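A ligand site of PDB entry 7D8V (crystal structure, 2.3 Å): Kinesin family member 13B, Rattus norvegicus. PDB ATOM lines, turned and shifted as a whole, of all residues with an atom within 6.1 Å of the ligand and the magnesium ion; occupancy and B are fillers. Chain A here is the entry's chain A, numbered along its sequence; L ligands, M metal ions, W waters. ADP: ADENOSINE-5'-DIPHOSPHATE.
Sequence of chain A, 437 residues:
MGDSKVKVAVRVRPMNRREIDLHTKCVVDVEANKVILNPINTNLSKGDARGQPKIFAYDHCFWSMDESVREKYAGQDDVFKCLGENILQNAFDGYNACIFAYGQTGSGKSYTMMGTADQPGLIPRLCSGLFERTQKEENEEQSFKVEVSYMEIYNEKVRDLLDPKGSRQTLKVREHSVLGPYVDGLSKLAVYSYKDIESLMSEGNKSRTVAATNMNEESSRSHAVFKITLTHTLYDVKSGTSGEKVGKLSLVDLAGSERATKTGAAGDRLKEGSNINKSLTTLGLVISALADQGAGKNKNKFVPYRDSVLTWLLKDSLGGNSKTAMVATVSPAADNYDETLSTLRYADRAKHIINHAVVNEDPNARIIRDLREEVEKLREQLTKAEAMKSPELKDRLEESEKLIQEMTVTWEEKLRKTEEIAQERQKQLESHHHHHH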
ATOM      1  N   ARG A  11      35.915  18.165  -3.349  1.00  0.00           N
ATOM      2  CA  ARG A  11      34.605  18.800  -3.327  1.00  0.00           C
ATOM      3  C   ARG A  11      34.255  19.247  -1.916  1.00  0.00           C
ATOM      4  O   ARG A  11      34.295  18.450  -0.973  1.00  0.00           O
ATOM      5  CB  ARG A  11      33.508  17.851  -3.818  1.00  0.00           C
ATOM      6  CG  ARG A  11      32.154  18.546  -3.882  1.00  0.00           C
ATOM      7  CD  ARG A  11      31.152  17.763  -4.712  1.00  0.00           C
ATOM      8  NE  ARG A  11      30.048  18.591  -5.199  1.00  0.00           N
ATOM      9  CZ  ARG A  11      28.938  18.081  -5.693  1.00  0.00           C
ATOM     10  NH1 ARG A  11      27.973  18.881  -6.147  1.00  0.00           N
ATOM     11  NH2 ARG A  11      28.796  16.747  -5.740  1.00  0.00           N
ATOM     12  N   VAL A  12      33.905  20.528  -1.777  1.00  0.00           N
ATOM     13  CA  VAL A  12      33.551  21.143  -0.504  1.00  0.00           C
ATOM     14  C   VAL A  12      32.030  21.231  -0.426  1.00  0.00           C
ATOM     15  O   VAL A  12      31.392  21.949  -1.206  1.00  0.00           O
ATOM     16  CB  VAL A  12      34.189  22.540  -0.374  1.00  0.00           C
ATOM     17  CG1 VAL A  12      33.910  23.118   1.031  1.00  0.00           C
ATOM     18  CG2 VAL A  12      35.675  22.468  -0.652  1.00  0.00           C
ATOM     19  N   ARG A  13      31.434  20.509   0.528  1.00  0.00           N
ATOM     20  CA  ARG A  13      29.981  20.496   0.664  1.00  0.00           C
ATOM     21  C   ARG A  13      29.505  21.763   1.370  1.00  0.00           C
ATOM     22  O   ARG A  13      30.301  22.487   1.969  1.00  0.00           O
ATOM     23  CB  ARG A  13      29.538  19.255   1.439  1.00  0.00           C
ATOM     24  CG  ARG A  13      29.972  19.202   2.914  1.00  0.00           C
ATOM     25  CD  ARG A  13      28.935  18.488   3.817  1.00  0.00           C
ATOM     26  NE  ARG A  13      27.605  19.100   3.725  1.00  0.00           N
ATOM     27  CZ  ARG A  13      26.524  18.706   4.400  1.00  0.00           C
ATOM     28  NH1 ARG A  13      26.593  17.666   5.235  1.00  0.00           N
ATOM     29  NH2 ARG A  13      25.381  19.341   4.239  1.00  0.00           N
ATOM     30  N   PRO A  14      28.207  22.059   1.309  1.00  0.00           N
ATOM     31  CA  PRO A  14      27.694  23.202   2.081  1.00  0.00           C
ATOM     32  C   PRO A  14      27.619  22.877   3.573  1.00  0.00           C
ATOM     33  O   PRO A  14      27.597  21.715   3.982  1.00  0.00           O
ATOM     34  CB  PRO A  14      26.299  23.441   1.496  1.00  0.00           C
ATOM     35  CG  PRO A  14      25.936  22.143   0.830  1.00  0.00           C
ATOM     36  CD  PRO A  14      27.208  21.543   0.357  1.00  0.00           C
ATOM     37  N   ASN A  16      26.054  22.071   6.925  1.00  0.00           N
ATOM     38  CA  ASN A  16      24.823  21.344   7.193  1.00  0.00           C
ATOM     39  C   ASN A  16      23.944  22.169   8.137  1.00  0.00           C
ATOM     40  O   ASN A  16      24.266  23.312   8.486  1.00  0.00           O
ATOM     41  CB  ASN A  16      25.125  19.925   7.705  1.00  0.00           C
ATOM     42  CG  ASN A  16      25.893  19.904   9.058  1.00  0.00           C
ATOM     43  OD1 ASN A  16      25.758  20.798   9.900  1.00  0.00           O
ATOM     44  ND2 ASN A  16      26.670  18.841   9.264  1.00  0.00           N
ATOM     45  N   SER A  64      30.961  23.707  -3.618  1.00  0.00           N
ATOM     46  CA  SER A  64      29.539  23.411  -3.722  1.00  0.00           C
ATOM     47  C   SER A  64      28.774  23.943  -2.516  1.00  0.00           C
ATOM     48  O   SER A  64      27.797  23.352  -2.065  1.00  0.00           O
ATOM     49  CB  SER A  64      29.310  21.911  -3.887  1.00  0.00           C
ATOM     50  OG  SER A  64      30.106  21.412  -4.941  1.00  0.00           O
ATOM     51  N   TYR A  73      30.043  28.240  -8.014  1.00  0.00           N
ATOM     52  CA  TYR A  73      29.397  27.056  -7.468  1.00  0.00           C
ATOM     53  C   TYR A  73      29.431  25.865  -8.445  1.00  0.00           C
ATOM     54  O   TYR A  73      29.050  25.995  -9.615  1.00  0.00           O
ATOM     55  CB  TYR A  73      27.935  27.407  -7.125  1.00  0.00           C
ATOM     56  CG  TYR A  73      27.102  26.221  -6.754  1.00  0.00           C
ATOM     57  CD1 TYR A  73      27.175  25.677  -5.482  1.00  0.00           C
ATOM     58  CD2 TYR A  73      26.238  25.642  -7.686  1.00  0.00           C
ATOM     59  CE1 TYR A  73      26.413  24.573  -5.140  1.00  0.00           C
ATOM     60  CE2 TYR A  73      25.463  24.538  -7.347  1.00  0.00           C
ATOM     61  CZ  TYR A  73      25.559  24.002  -6.079  1.00  0.00           C
ATOM     62  OH  TYR A  73      24.802  22.910  -5.731  1.00  0.00           O
ATOM     63  N   ALA A  74      29.852  24.700  -7.940  1.00  0.00           N
ATOM     64  CA  ALA A  74      29.848  23.453  -8.689  1.00  0.00           C
ATOM     65  C   ALA A  74      28.657  22.606  -8.256  1.00  0.00           C
ATOM     66  O   ALA A  74      28.619  22.110  -7.123  1.00  0.00           O
ATOM     67  CB  ALA A  74      31.159  22.697  -8.488  1.00  0.00           C
ATOM     68  N   GLY A 103      36.304  10.424   2.150  1.00  0.00           N
ATOM     69  CA  GLY A 103      36.145  11.514   3.085  1.00  0.00           C
ATOM     70  C   GLY A 103      35.310  11.118   4.284  1.00  0.00           C
ATOM     71  O   GLY A 103      34.708  10.044   4.332  1.00  0.00           O
ATOM     72  N   GLN A 104      35.288  12.009   5.274  1.00  0.00           N
ATOM     73  CA  GLN A 104      34.599  11.693   6.519  1.00  0.00           C
ATOM     74  C   GLN A 104      33.096  11.542   6.293  1.00  0.00           C
ATOM     75  O   GLN A 104      32.531  12.054   5.322  1.00  0.00           O
ATOM     76  CB  GLN A 104      34.896  12.748   7.587  1.00  0.00           C
ATOM     77  CG  GLN A 104      34.052  14.019   7.543  1.00  0.00           C
ATOM     78  CD  GLN A 104      34.432  14.993   8.667  1.00  0.00           C
ATOM     79  OE1 GLN A 104      34.907  16.105   8.409  1.00  0.00           O
ATOM     80  NE2 GLN A 104      34.230  14.580   9.912  1.00  0.00           N
ATOM     81  N   THR A 105      32.459  10.794   7.182  1.00  0.00           N
ATOM     82  CA  THR A 105      31.005  10.647   7.153  1.00  0.00           C
ATOM     83  C   THR A 105      30.337  12.025   7.179  1.00  0.00           C
ATOM     84  O   THR A 105      30.656  12.880   8.001  1.00  0.00           O
ATOM     85  CB  THR A 105      30.542   9.825   8.352  1.00  0.00           C
ATOM     86  OG1 THR A 105      31.140   8.520   8.276  1.00  0.00           O
ATOM     87  CG2 THR A 105      29.003   9.664   8.365  1.00  0.00           C
ATOM     88  N   GLY A 106      29.395  12.213   6.255  1.00  0.00           N
ATOM     89  CA  GLY A 106      28.670  13.463   6.158  1.00  0.00           C
ATOM     90  C   GLY A 106      29.277  14.486   5.237  1.00  0.00           C
ATOM     91  O   GLY A 106      28.700  15.572   5.073  1.00  0.00           O
ATOM     92  N   SER A 107      30.407  14.179   4.602  1.00  0.00           N
ATOM     93  CA  SER A 107      31.094  15.179   3.795  1.00  0.00           C
ATOM     94  C   SER A 107      30.648  15.176   2.342  1.00  0.00           C
ATOM     95  O   SER A 107      31.011  16.108   1.602  1.00  0.00           O
ATOM     96  CB  SER A 107      32.612  14.964   3.848  1.00  0.00           C
ATOM     97  OG  SER A 107      32.956  13.699   3.303  1.00  0.00           O
ATOM     98  N   GLY A 108      29.931  14.159   1.895  1.00  0.00           N
ATOM     99  CA  GLY A 108      29.328  14.205   0.582  1.00  0.00           C
ATOM    100  C   GLY A 108      29.713  13.100  -0.400  1.00  0.00           C
ATOM    101  O   GLY A 108      29.508  13.285  -1.605  1.00  0.00           O
ATOM    102  N   LYS A 109      30.243  11.971   0.102  1.00  0.00           N
ATOM    103  CA  LYS A 109      30.655  10.867  -0.764  1.00  0.00           C
ATOM    104  C   LYS A 109      29.467  10.304  -1.555  1.00  0.00           C
ATOM    105  O   LYS A 109      29.544  10.133  -2.784  1.00  0.00           O
ATOM    106  CB  LYS A 109      31.293   9.736   0.068  1.00  0.00           C
ATOM    107  CG  LYS A 109      32.672  10.050   0.646  1.00  0.00           C
ATOM    108  CD  LYS A 109      33.251   8.876   1.429  1.00  0.00           C
ATOM    109  CE  LYS A 109      32.305   8.411   2.556  1.00  0.00           C
ATOM    110  NZ  LYS A 109      31.987   9.515   3.510  1.00  0.00           N
ATOM    111  N   SER A 110      28.377   9.980  -0.858  1.00  0.00           N
ATOM    112  CA  SER A 110      27.207   9.410  -1.526  1.00  0.00           C
ATOM    113  C   SER A 110      26.487  10.448  -2.369  1.00  0.00           C
ATOM    114  O   SER A 110      25.996  10.126  -3.459  1.00  0.00           O
ATOM    115  CB  SER A 110      26.239   8.804  -0.492  1.00  0.00           C
ATOM    116  OG  SER A 110      26.852   7.765   0.259  1.00  0.00           O
ATOM    117  N   TYR A 111      26.354  11.679  -1.869  1.00  0.00           N
ATOM    118  CA  TYR A 111      25.736  12.738  -2.658  1.00  0.00           C
ATOM    119  C   TYR A 111      26.468  12.913  -3.986  1.00  0.00           C
ATOM    120  O   TYR A 111      25.843  13.204  -5.006  1.00  0.00           O
ATOM    121  CB  TYR A 111      25.719  14.050  -1.867  1.00  0.00           C
ATOM    122  CG  TYR A 111      25.098  15.191  -2.628  1.00  0.00           C
ATOM    123  CD1 TYR A 111      23.730  15.434  -2.563  1.00  0.00           C
ATOM    124  CD2 TYR A 111      25.866  16.036  -3.418  1.00  0.00           C
ATOM    125  CE1 TYR A 111      23.152  16.479  -3.252  1.00  0.00           C
ATOM    126  CE2 TYR A 111      25.305  17.078  -4.117  1.00  0.00           C
ATOM    127  CZ  TYR A 111      23.941  17.294  -4.034  1.00  0.00           C
ATOM    128  OH  TYR A 111      23.379  18.326  -4.730  1.00  0.00           O
ATOM    129  N   THR A 112      27.776  12.689  -3.997  1.00  0.00           N
ATOM    130  CA  THR A 112      28.586  12.871  -5.183  1.00  0.00           C
ATOM    131  C   THR A 112      28.510  11.661  -6.101  1.00  0.00           C
ATOM    132  O   THR A 112      28.468  11.808  -7.333  1.00  0.00           O
ATOM    133  CB  THR A 112      30.036  13.130  -4.775  1.00  0.00           C
ATOM    134  OG1 THR A 112      30.113  14.402  -4.137  1.00  0.00           O
ATOM    135  CG2 THR A 112      30.965  13.155  -5.977  1.00  0.00           C
ATOM    136  N   THR A 116      20.887  12.430  -4.843  1.00  0.00           N
ATOM    137  CA  THR A 116      19.496  12.276  -4.430  1.00  0.00           C
ATOM    138  C   THR A 116      18.592  12.268  -5.658  1.00  0.00           C
ATOM    139  O   THR A 116      19.008  12.570  -6.785  1.00  0.00           O
ATOM    140  CB  THR A 116      19.107  13.398  -3.463  1.00  0.00           C
ATOM    141  OG1 THR A 116      19.091  14.640  -4.169  1.00  0.00           O
ATOM    142  CG2 THR A 116      20.124  13.491  -2.313  1.00  0.00           C
ATOM    143  N   ARG A 208      21.124  -1.168   0.327  1.00  0.00           N
ATOM    144  CA  ARG A 208      22.049  -0.407   1.173  1.00  0.00           C
ATOM    145  C   ARG A 208      21.315   0.224   2.333  1.00  0.00           C
ATOM    146  O   ARG A 208      21.841   0.303   3.456  1.00  0.00           O
ATOM    147  CB  ARG A 208      22.787   0.679   0.384  1.00  0.00           C
ATOM    148  CG  ARG A 208      23.924   0.202  -0.472  1.00  0.00           C
ATOM    149  CD  ARG A 208      25.260   0.121   0.285  1.00  0.00           C
ATOM    150  NE  ARG A 208      25.948   1.367   0.652  1.00  0.00           N
ATOM    151  CZ  ARG A 208      26.057   2.477  -0.092  1.00  0.00           C
ATOM    152  NH1 ARG A 208      26.744   3.503   0.382  1.00  0.00           N
ATOM    153  NH2 ARG A 208      25.502   2.575  -1.293  1.00  0.00           N
ATOM    154  N   SER A 219      26.446   1.645   9.040  1.00  0.00           N
ATOM    155  CA  SER A 219      26.371   1.837   7.601  1.00  0.00           C
ATOM    156  C   SER A 219      27.365   2.876   7.114  1.00  0.00           C
ATOM    157  O   SER A 219      27.711   2.882   5.929  1.00  0.00           O
ATOM    158  CB  SER A 219      24.950   2.208   7.174  1.00  0.00           C
ATOM    159  OG  SER A 219      24.520   3.407   7.799  1.00  0.00           O
ATOM    160  N   ASP A 253      32.147   4.160  -3.439  1.00  0.00           N
ATOM    161  CA  ASP A 253      31.653   5.042  -2.381  1.00  0.00           C
ATOM    162  C   ASP A 253      32.220   4.432  -1.109  1.00  0.00           C
ATOM    163  O   ASP A 253      31.706   3.416  -0.639  1.00  0.00           O
ATOM    164  CB  ASP A 253      30.117   5.100  -2.404  1.00  0.00           C
ATOM    165  CG  ASP A 253      29.518   6.029  -1.345  1.00  0.00           C
ATOM    166  OD1 ASP A 253      30.243   6.569  -0.463  1.00  0.00           O
ATOM    167  OD2 ASP A 253      28.271   6.192  -1.389  1.00  0.00           O
ATOM    168  N   LEU A 254      33.290   5.015  -0.588  1.00  0.00           N
ATOM    169  CA  LEU A 254      34.039   4.366   0.479  1.00  0.00           C
ATOM    170  C   LEU A 254      33.334   4.531   1.831  1.00  0.00           C
ATOM    171  O   LEU A 254      32.348   5.258   1.969  1.00  0.00           O
ATOM    172  CB  LEU A 254      35.470   4.921   0.543  1.00  0.00           C
ATOM    173  CG  LEU A 254      36.417   4.619  -0.629  1.00  0.00           C
ATOM    174  CD1 LEU A 254      37.693   5.446  -0.486  1.00  0.00           C
ATOM    175  CD2 LEU A 254      36.772   3.148  -0.707  1.00  0.00           C
ATOM    176  N   THR A 329      36.065  14.414  -0.557  1.00  0.00           N
ATOM    177  CA  THR A 329      34.960  15.273  -0.133  1.00  0.00           C
ATOM    178  C   THR A 329      35.251  15.789   1.262  1.00  0.00           C
ATOM    179  O   THR A 329      35.649  15.021   2.151  1.00  0.00           O
ATOM    180  CB  THR A 329      33.613  14.536  -0.163  1.00  0.00           C
ATOM    181  OG1 THR A 329      33.725  13.306   0.567  1.00  0.00           O
ATOM    182  CG2 THR A 329      33.172  14.226  -1.595  1.00  0.00           C
HETATM  183  PB  ADP L   1      28.586  10.762   3.139  1.00  0.00           P
HETATM  184  O1B ADP L   1      28.027   9.780   2.136  1.00  0.00           O
HETATM  185  O2B ADP L   1      28.374  10.355   4.579  1.00  0.00           O
HETATM  186  O3B ADP L   1      30.005  11.214   2.856  1.00  0.00           O
HETATM  187  PA  ADP L   1      26.368  12.266   2.142  1.00  0.00           P
HETATM  188  O1A ADP L   1      26.648  12.290   0.656  1.00  0.00           O
HETATM  189  O2A ADP L   1      25.414  11.251   2.717  1.00  0.00           O
HETATM  190  O3A ADP L   1      27.778  12.147   2.924  1.00  0.00           O
HETATM  191  O5' ADP L   1      25.912  13.747   2.587  1.00  0.00           O
HETATM  192  C5' ADP L   1      25.185  13.945   3.800  1.00  0.00           C
HETATM  193  C4' ADP L   1      24.040  14.912   3.527  1.00  0.00           C
HETATM  194  O4' ADP L   1      24.554  16.157   3.055  1.00  0.00           O
HETATM  195  C3' ADP L   1      23.130  14.341   2.441  1.00  0.00           C
HETATM  196  O3' ADP L   1      21.786  14.346   2.903  1.00  0.00           O
HETATM  197  C2' ADP L   1      23.274  15.281   1.269  1.00  0.00           C
HETATM  198  O2' ADP L   1      21.990  15.561   0.702  1.00  0.00           O
HETATM  199  C1' ADP L   1      23.925  16.531   1.823  1.00  0.00           C
HETATM  200  N9  ADP L   1      24.978  16.988   0.898  1.00  0.00           N
HETATM  201  C8  ADP L   1      26.200  16.432   0.812  1.00  0.00           C
HETATM  202  N7  ADP L   1      26.958  17.065  -0.130  1.00  0.00           N
HETATM  203  C5  ADP L   1      26.206  18.041  -0.662  1.00  0.00           C
HETATM  204  C6  ADP L   1      26.403  19.083  -1.691  1.00  0.00           C
HETATM  205  N6  ADP L   1      27.580  19.202  -2.361  1.00  0.00           N
HETATM  206  N1  ADP L   1      25.362  19.912  -1.953  1.00  0.00           N
HETATM  207  C2  ADP L   1      24.195  19.810  -1.293  1.00  0.00           C
HETATM  208  N3  ADP L   1      23.958  18.892  -0.345  1.00  0.00           N
HETATM  209  C4  ADP L   1      24.905  17.996   0.026  1.00  0.00           C
HETATM  210 MG    MG M   1      27.087   7.702   2.332  1.00  0.00          MG
HETATM  211  O   HOH W   1      28.950   6.900   1.944  1.00  0.00           O
HETATM  212  O   HOH W   2      26.180  10.623   5.892  1.00  0.00           O
HETATM  213  O   HOH W   3      25.435   8.945   2.727  1.00  0.00           O
HETATM  214  O   HOH W   4      27.950   7.584   4.501  1.00  0.00           O
HETATM  215  O   HOH W   5      29.091  17.062  -1.895  1.00  0.00           O
HETATM  216  O   HOH W   6      26.386   5.704   2.556  1.00  0.00           O
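O1A of the ligand sits at hydrogen-bond distance from N of Ser 110, 3.3 Å away.
N of Tyr 111 is in hydrogen-bond range of O1A of the ligand.
N of Lys 109 is in hydrogen-bond range of O3B of the ligand, 2.9 Å away.
The side-chain amino group of Lys 109 lies within salt-bridge range of an oxygen (O3B) of the ligand (2.7 Å).
N of Gly 106 is in hydrogen-bond range of O2B of the ligand (2.7 Å).
An oxygen (O3B) of the ligand sits at hydrogen-bond distance from the backbone NH (N) of Gly 108, 3.1 Å away.
The guanidinium group (NH1) of Arg 13 lies within hydrogen-bond range of an oxygen (O4') of the ligand.
An oxygen (O3B) of the ligand is in hydrogen-bond range of the backbone NH (N) of Ser 107 (3.5 Å).
The side-chain amino group of Lys 109 is in hydrogen-bond range of the backbone carbonyl oxygen of Gln 104.
The backbone carbonyl oxygen (O) of Gly 103 is in hydrogen-bond range of the side-chain amino group (NZ) of Lys 109 (2.9 Å).
The backbone carbonyl oxygen of Gly 106 is in hydrogen-bond range of the guanidinium group of Arg 13.
OG1 of Thr 112 lies within hydrogen-bond range of O of Gly 108.
The side-chain hydroxyl (OG) of Ser 107 sits at hydrogen-bond distance from the backbone carbonyl oxygen (O) of Gln 104 (2.6 Å).
OG1 of Thr 329 sits at hydrogen-bond distance from OG of Ser 107 (2.9 Å).
NE of Arg 11 lies within hydrogen-bond range of OG of Ser 64, at 2.8 Å.
O of Ala 74 lies within hydrogen-bond range of NH1 of Arg 11 (3.4 Å).
CZ of Arg 11 touches N6 of the ligand, 3.8 Å away.
Pro 14 touches the ligand (CD to C6, 3.3 Å).
Ser 64 touches the ligand.
Gln 104 touches the ligand.
Thr 105 touches the ligand.
The nearest printed residue that does not touch the ligand is Thr 116 (4.1 Å).
Of the 24 residues printed, 1 comes within 4 Å of the magnesium ion.
The magnesium ion is bound by water W1 (2.1 Å), OG of Ser 110 (2.1 Å), water W3 (2.1 Å), water W6 (2.1 Å), O1B of the ligand (2.3 Å) and water W4 (2.3 Å).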
